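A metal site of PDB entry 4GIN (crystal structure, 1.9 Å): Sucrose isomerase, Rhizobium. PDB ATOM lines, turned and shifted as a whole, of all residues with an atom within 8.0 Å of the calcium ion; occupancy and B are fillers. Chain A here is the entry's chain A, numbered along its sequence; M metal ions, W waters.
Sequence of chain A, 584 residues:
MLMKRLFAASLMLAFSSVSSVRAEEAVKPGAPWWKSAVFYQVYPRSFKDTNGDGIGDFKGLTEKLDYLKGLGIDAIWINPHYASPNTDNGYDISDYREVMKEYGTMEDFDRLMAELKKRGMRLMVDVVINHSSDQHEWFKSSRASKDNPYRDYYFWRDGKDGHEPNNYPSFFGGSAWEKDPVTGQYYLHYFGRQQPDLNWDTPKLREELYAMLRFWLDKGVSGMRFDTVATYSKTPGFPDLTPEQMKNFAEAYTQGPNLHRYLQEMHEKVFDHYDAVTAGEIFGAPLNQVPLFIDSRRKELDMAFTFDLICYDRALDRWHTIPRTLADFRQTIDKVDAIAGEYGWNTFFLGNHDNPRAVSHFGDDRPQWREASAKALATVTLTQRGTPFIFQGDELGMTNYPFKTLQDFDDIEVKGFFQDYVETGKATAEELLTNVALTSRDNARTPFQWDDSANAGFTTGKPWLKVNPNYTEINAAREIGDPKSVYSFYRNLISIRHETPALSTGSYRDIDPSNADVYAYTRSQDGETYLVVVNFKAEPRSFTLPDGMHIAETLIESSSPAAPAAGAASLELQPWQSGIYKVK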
ATOM      1  N   PRO A  44     -23.307 -24.075  -4.940  1.00  0.00           N
ATOM      2  CA  PRO A  44     -23.745 -22.726  -4.524  1.00  0.00           C
ATOM      3  C   PRO A  44     -23.289 -21.628  -5.477  1.00  0.00           C
ATOM      4  O   PRO A  44     -24.023 -20.672  -5.674  1.00  0.00           O
ATOM      5  CB  PRO A  44     -23.100 -22.556  -3.154  1.00  0.00           C
ATOM      6  CG  PRO A  44     -22.904 -23.948  -2.651  1.00  0.00           C
ATOM      7  CD  PRO A  44     -22.546 -24.756  -3.882  1.00  0.00           C
ATOM      8  N   ARG A  45     -22.117 -21.804  -6.077  1.00  0.00           N
ATOM      9  CA  ARG A  45     -21.573 -20.863  -7.071  1.00  0.00           C
ATOM     10  C   ARG A  45     -22.538 -20.529  -8.199  1.00  0.00           C
ATOM     11  O   ARG A  45     -22.539 -19.406  -8.712  1.00  0.00           O
ATOM     12  CB  ARG A  45     -20.268 -21.428  -7.642  1.00  0.00           C
ATOM     13  CG  ARG A  45     -19.707 -20.659  -8.840  1.00  0.00           C
ATOM     14  CD  ARG A  45     -18.281 -21.104  -9.195  1.00  0.00           C
ATOM     15  NE  ARG A  45     -17.334 -20.421  -8.314  1.00  0.00           N
ATOM     16  CZ  ARG A  45     -16.736 -19.271  -8.614  1.00  0.00           C
ATOM     17  NH1 ARG A  45     -15.914 -18.717  -7.733  1.00  0.00           N
ATOM     18  NH2 ARG A  45     -16.949 -18.676  -9.785  1.00  0.00           N
ATOM     19  N   LYS A  48     -27.781 -19.063  -6.517  1.00  0.00           N
ATOM     20  CA  LYS A  48     -28.362 -17.714  -6.417  1.00  0.00           C
ATOM     21  C   LYS A  48     -27.372 -16.694  -5.868  1.00  0.00           C
ATOM     22  O   LYS A  48     -26.857 -16.843  -4.756  1.00  0.00           O
ATOM     23  CB  LYS A  48     -29.632 -17.726  -5.556  1.00  0.00           C
ATOM     24  CG  LYS A  48     -30.313 -16.362  -5.400  1.00  0.00           C
ATOM     25  CD  LYS A  48     -30.909 -15.861  -6.722  1.00  0.00           C
ATOM     26  CE  LYS A  48     -31.783 -14.622  -6.527  1.00  0.00           C
ATOM     27  NZ  LYS A  48     -31.012 -13.428  -6.053  1.00  0.00           N
ATOM     28  N   ASP A  49     -27.110 -15.653  -6.659  1.00  0.00           N
ATOM     29  CA  ASP A  49     -26.230 -14.563  -6.256  1.00  0.00           C
ATOM     30  C   ASP A  49     -27.073 -13.459  -5.601  1.00  0.00           C
ATOM     31  O   ASP A  49     -28.114 -13.067  -6.144  1.00  0.00           O
ATOM     32  CB  ASP A  49     -25.545 -14.003  -7.512  1.00  0.00           C
ATOM     33  CG  ASP A  49     -24.648 -12.806  -7.227  1.00  0.00           C
ATOM     34  OD1 ASP A  49     -24.222 -12.624  -6.060  1.00  0.00           O
ATOM     35  OD2 ASP A  49     -24.341 -12.048  -8.182  1.00  0.00           O
ATOM     36  N   THR A  50     -26.640 -12.942  -4.438  1.00  0.00           N
ATOM     37  CA  THR A  50     -27.399 -11.869  -3.790  1.00  0.00           C
ATOM     38  C   THR A  50     -26.640 -10.541  -3.653  1.00  0.00           C
ATOM     39  O   THR A  50     -27.154  -9.594  -3.055  1.00  0.00           O
ATOM     40  CB  THR A  50     -27.852 -12.258  -2.378  1.00  0.00           C
ATOM     41  OG1 THR A  50     -26.726 -12.721  -1.623  1.00  0.00           O
ATOM     42  CG2 THR A  50     -28.918 -13.349  -2.439  1.00  0.00           C
ATOM     43  N   ASN A  51     -25.426 -10.461  -4.179  1.00  0.00           N
ATOM     44  CA  ASN A  51     -24.703  -9.183  -4.062  1.00  0.00           C
ATOM     45  C   ASN A  51     -24.138  -8.662  -5.378  1.00  0.00           C
ATOM     46  O   ASN A  51     -23.292  -7.783  -5.391  1.00  0.00           O
ATOM     47  CB  ASN A  51     -23.603  -9.266  -2.995  1.00  0.00           C
ATOM     48  CG  ASN A  51     -22.422 -10.121  -3.434  1.00  0.00           C
ATOM     49  OD1 ASN A  51     -22.560 -11.020  -4.272  1.00  0.00           O
ATOM     50  ND2 ASN A  51     -21.263  -9.851  -2.862  1.00  0.00           N
ATOM     51  N   GLY A  52     -24.620  -9.233  -6.477  1.00  0.00           N
ATOM     52  CA  GLY A  52     -24.265  -8.743  -7.800  1.00  0.00           C
ATOM     53  C   GLY A  52     -22.850  -9.022  -8.307  1.00  0.00           C
ATOM     54  O   GLY A  52     -22.472  -8.459  -9.322  1.00  0.00           O
ATOM     55  N   ASP A  53     -22.082  -9.888  -7.632  1.00  0.00           N
ATOM     56  CA  ASP A  53     -20.731 -10.220  -8.126  1.00  0.00           C
ATOM     57  C   ASP A  53     -20.734 -11.338  -9.172  1.00  0.00           C
ATOM     58  O   ASP A  53     -19.685 -11.702  -9.705  1.00  0.00           O
ATOM     59  CB  ASP A  53     -19.751 -10.513  -6.988  1.00  0.00           C
ATOM     60  CG  ASP A  53     -20.129 -11.748  -6.184  1.00  0.00           C
ATOM     61  OD1 ASP A  53     -21.180 -12.364  -6.443  1.00  0.00           O
ATOM     62  OD2 ASP A  53     -19.379 -12.092  -5.253  1.00  0.00           O
ATOM     63  N   GLY A  54     -21.916 -11.899  -9.455  1.00  0.00           N
ATOM     64  CA  GLY A  54     -22.051 -12.923 -10.482  1.00  0.00           C
ATOM     65  C   GLY A  54     -21.781 -14.330  -9.970  1.00  0.00           C
ATOM     66  O   GLY A  54     -21.782 -15.306 -10.740  1.00  0.00           O
ATOM     67  N   ILE A  55     -21.560 -14.430  -8.658  1.00  0.00           N
ATOM     68  CA  ILE A  55     -21.288 -15.720  -8.042  1.00  0.00           C
ATOM     69  C   ILE A  55     -22.345 -16.023  -6.989  1.00  0.00           C
ATOM     70  O   ILE A  55     -22.658 -15.162  -6.154  1.00  0.00           O
ATOM     71  CB  ILE A  55     -19.897 -15.708  -7.388  1.00  0.00           C
ATOM     72  CG1 ILE A  55     -18.827 -15.442  -8.452  1.00  0.00           C
ATOM     73  CG2 ILE A  55     -19.631 -17.020  -6.621  1.00  0.00           C
ATOM     74  CD1 ILE A  55     -17.420 -15.297  -7.898  1.00  0.00           C
ATOM     75  N   GLY A  56     -22.909 -17.224  -7.020  1.00  0.00           N
ATOM     76  CA  GLY A  56     -23.943 -17.603  -6.062  1.00  0.00           C
ATOM     77  C   GLY A  56     -23.348 -17.655  -4.663  1.00  0.00           C
ATOM     78  O   GLY A  56     -22.136 -17.879  -4.510  1.00  0.00           O
ATOM     79  N   ASP A  57     -24.176 -17.469  -3.630  1.00  0.00           N
ATOM     80  CA  ASP A  57     -23.665 -17.365  -2.263  1.00  0.00           C
ATOM     81  C   ASP A  57     -24.622 -17.978  -1.220  1.00  0.00           C
ATOM     82  O   ASP A  57     -25.730 -18.434  -1.555  1.00  0.00           O
ATOM     83  CB  ASP A  57     -23.377 -15.889  -1.942  1.00  0.00           C
ATOM     84  CG  ASP A  57     -24.500 -14.983  -2.413  1.00  0.00           C
ATOM     85  OD1 ASP A  57     -25.600 -15.048  -1.823  1.00  0.00           O
ATOM     86  OD2 ASP A  57     -24.296 -14.204  -3.372  1.00  0.00           O
ATOM     87  N   PHE A  58     -24.194 -17.990   0.041  1.00  0.00           N
ATOM     88  CA  PHE A  58     -25.010 -18.577   1.118  1.00  0.00           C
ATOM     89  C   PHE A  58     -26.346 -17.855   1.266  1.00  0.00           C
ATOM     90  O   PHE A  58     -27.383 -18.474   1.473  1.00  0.00           O
ATOM     91  CB  PHE A  58     -24.296 -18.488   2.469  1.00  0.00           C
ATOM     92  CG  PHE A  58     -23.088 -19.387   2.609  1.00  0.00           C
ATOM     93  CD1 PHE A  58     -23.114 -20.692   2.150  1.00  0.00           C
ATOM     94  CD2 PHE A  58     -21.948 -18.928   3.244  1.00  0.00           C
ATOM     95  CE1 PHE A  58     -22.006 -21.521   2.300  1.00  0.00           C
ATOM     96  CE2 PHE A  58     -20.831 -19.743   3.385  1.00  0.00           C
ATOM     97  CZ  PHE A  58     -20.868 -21.049   2.927  1.00  0.00           C
ATOM     98  N   LYS A  59     -26.310 -16.521   1.212  1.00  0.00           N
ATOM     99  CA  LYS A  59     -27.531 -15.742   1.384  1.00  0.00           C
ATOM    100  C   LYS A  59     -28.545 -16.100   0.285  1.00  0.00           C
ATOM    101  O   LYS A  59     -29.753 -16.162   0.523  1.00  0.00           O
ATOM    102  CB  LYS A  59     -27.182 -14.241   1.340  1.00  0.00           C
ATOM    103  CG  LYS A  59     -28.339 -13.318   1.658  1.00  0.00           C
ATOM    104  CD  LYS A  59     -27.901 -11.854   1.668  1.00  0.00           C
ATOM    105  CE  LYS A  59     -26.680 -11.645   2.560  1.00  0.00           C
ATOM    106  NZ  LYS A  59     -26.357 -10.189   2.777  1.00  0.00           N
ATOM    107  N   GLY A  60     -28.037 -16.335  -0.925  1.00  0.00           N
ATOM    108  CA  GLY A  60     -28.888 -16.723  -2.040  1.00  0.00           C
ATOM    109  C   GLY A  60     -29.569 -18.058  -1.822  1.00  0.00           C
ATOM    110  O   GLY A  60     -30.782 -18.203  -2.074  1.00  0.00           O
ATOM    111  N   LYS A 101     -14.765 -17.709   1.183  1.00  0.00           N
ATOM    112  CA  LYS A 101     -15.054 -16.265   1.171  1.00  0.00           C
ATOM    113  C   LYS A 101     -16.058 -15.835   0.093  1.00  0.00           C
ATOM    114  O   LYS A 101     -16.892 -14.943   0.348  1.00  0.00           O
ATOM    115  CB  LYS A 101     -13.752 -15.453   1.050  1.00  0.00           C
ATOM    116  N   GLU A 102     -16.004 -16.451  -1.086  1.00  0.00           N
ATOM    117  CA  GLU A 102     -16.947 -16.099  -2.160  1.00  0.00           C
ATOM    118  C   GLU A 102     -18.413 -16.359  -1.800  1.00  0.00           C
ATOM    119  O   GLU A 102     -19.306 -15.700  -2.341  1.00  0.00           O
ATOM    120  CB  GLU A 102     -16.631 -16.852  -3.455  1.00  0.00           C
ATOM    121  CG  GLU A 102     -15.431 -16.314  -4.211  1.00  0.00           C
ATOM    122  CD  GLU A 102     -14.127 -16.873  -3.678  1.00  0.00           C
ATOM    123  OE1 GLU A 102     -14.162 -17.734  -2.770  1.00  0.00           O
ATOM    124  OE2 GLU A 102     -13.076 -16.459  -4.191  1.00  0.00           O
ATOM    125  N   TYR A 103     -18.650 -17.309  -0.915  1.00  0.00           N
ATOM    126  CA  TYR A 103     -20.023 -17.643  -0.513  1.00  0.00           C
ATOM    127  C   TYR A 103     -20.570 -16.763   0.613  1.00  0.00           C
ATOM    128  O   TYR A 103     -21.771 -16.729   0.845  1.00  0.00           O
ATOM    129  CB  TYR A 103     -20.097 -19.104  -0.092  1.00  0.00           C
ATOM    130  CG  TYR A 103     -19.878 -20.044  -1.240  1.00  0.00           C
ATOM    131  CD1 TYR A 103     -19.910 -19.599  -2.554  1.00  0.00           C
ATOM    132  CD2 TYR A 103     -19.645 -21.398  -1.012  1.00  0.00           C
ATOM    133  CE1 TYR A 103     -19.711 -20.491  -3.624  1.00  0.00           C
ATOM    134  CE2 TYR A 103     -19.457 -22.276  -2.056  1.00  0.00           C
ATOM    135  CZ  TYR A 103     -19.480 -21.813  -3.356  1.00  0.00           C
ATOM    136  OH  TYR A 103     -19.296 -22.720  -4.377  1.00  0.00           O
ATOM    137  N   GLY A 104     -19.682 -16.106   1.337  1.00  0.00           N
ATOM    138  CA  GLY A 104     -20.103 -15.271   2.448  1.00  0.00           C
ATOM    139  C   GLY A 104     -19.261 -15.452   3.692  1.00  0.00           C
ATOM    140  O   GLY A 104     -18.052 -15.694   3.612  1.00  0.00           O
ATOM    141  N   PHE A 458     -30.700 -14.810 -11.812  1.00  0.00           N
ATOM    142  CA  PHE A 458     -29.635 -15.396 -11.011  1.00  0.00           C
ATOM    143  C   PHE A 458     -28.802 -14.337 -10.330  1.00  0.00           C
ATOM    144  O   PHE A 458     -28.329 -14.552  -9.221  1.00  0.00           O
ATOM    145  CB  PHE A 458     -28.718 -16.255 -11.880  1.00  0.00           C
ATOM    146  CG  PHE A 458     -27.395 -16.583 -11.235  1.00  0.00           C
ATOM    147  CD1 PHE A 458     -27.314 -17.479 -10.193  1.00  0.00           C
ATOM    148  CD2 PHE A 458     -26.223 -15.988 -11.713  1.00  0.00           C
ATOM    149  CE1 PHE A 458     -26.090 -17.781  -9.603  1.00  0.00           C
ATOM    150  CE2 PHE A 458     -24.999 -16.297 -11.136  1.00  0.00           C
ATOM    151  CZ  PHE A 458     -24.918 -17.194 -10.093  1.00  0.00           C
ATOM    152  N   THR A 459     -28.613 -13.210 -11.007  1.00  0.00           N
ATOM    153  CA  THR A 459     -27.745 -12.143 -10.526  1.00  0.00           C
ATOM    154  C   THR A 459     -28.144 -10.823 -11.151  1.00  0.00           C
ATOM    155  O   THR A 459     -28.694 -10.787 -12.247  1.00  0.00           O
ATOM    156  CB  THR A 459     -26.262 -12.402 -10.889  1.00  0.00           C
ATOM    157  OG1 THR A 459     -25.449 -11.349 -10.343  1.00  0.00           O
ATOM    158  CG2 THR A 459     -26.062 -12.460 -12.404  1.00  0.00           C
HETATM  159 CA    CA M   1     -22.425 -13.304  -4.676  1.00  0.00          CA
HETATM  160  O   HOH W   1     -20.515 -14.440  -4.195  1.00  0.00           O
HETATM  161  O   HOH W   2     -21.694 -13.135  -2.254  1.00  0.00           O
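The side-chain carboxylate (OD2) of Asp 49 sits at hydrogen-bond distance from the backbone NH (N) of Gly 54 (2.7 Å). OD2 of Asp 49 lies within hydrogen-bond range of N of Gly 52 (3.3 Å). The backbone NH (N) of Asp 57 sits at hydrogen-bond distance from the backbone carbonyl oxygen (O) of Lys 48 (3.0 Å). The backbone NH of Asp 49 lies within hydrogen-bond range of the backbone carbonyl oxygen of Phe 458 (3.0 Å). The side-chain carboxylate (OD1) of Asp 57 is in hydrogen-bond range of the backbone NH (N) of Gly 60 (2.9 Å). The side-chain hydroxyl (OG1) of Thr 459 sits at hydrogen-bond distance from the side-chain carboxylate (OD2) of Asp 49, 2.5 Å away. The side-chain carboxylate (OD1) of Asp 57 sits close to the backbone NH (N) of Lys 59 (3.4 Å). OD1 of Asp 57 is in hydrogen-bond range of OG1 of Thr 50 (2.6 Å).
The calcium ion is bound by water W1 (2.3 Å), the side-chain amide oxygen of Asn 51 (2.3 Å), the side-chain carboxylate of Asp 53 (2.4 Å), the side-chain carboxylate of Asp 49 (2.4 Å), the backbone carbonyl oxygen of Ile 55 (2.4 Å), the side-chain carboxylate of Asp 57 (2.5 Å) and water W2 (2.5 Å). The calcium ion has seven donor atoms within binding distance.
Water W1 lies within hydrogen-bond range of the backbone carbonyl oxygen (O) of Glu 102 (2.5 Å) and the side-chain carboxylate (OD2) of Asp 53 (2.8 Å).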
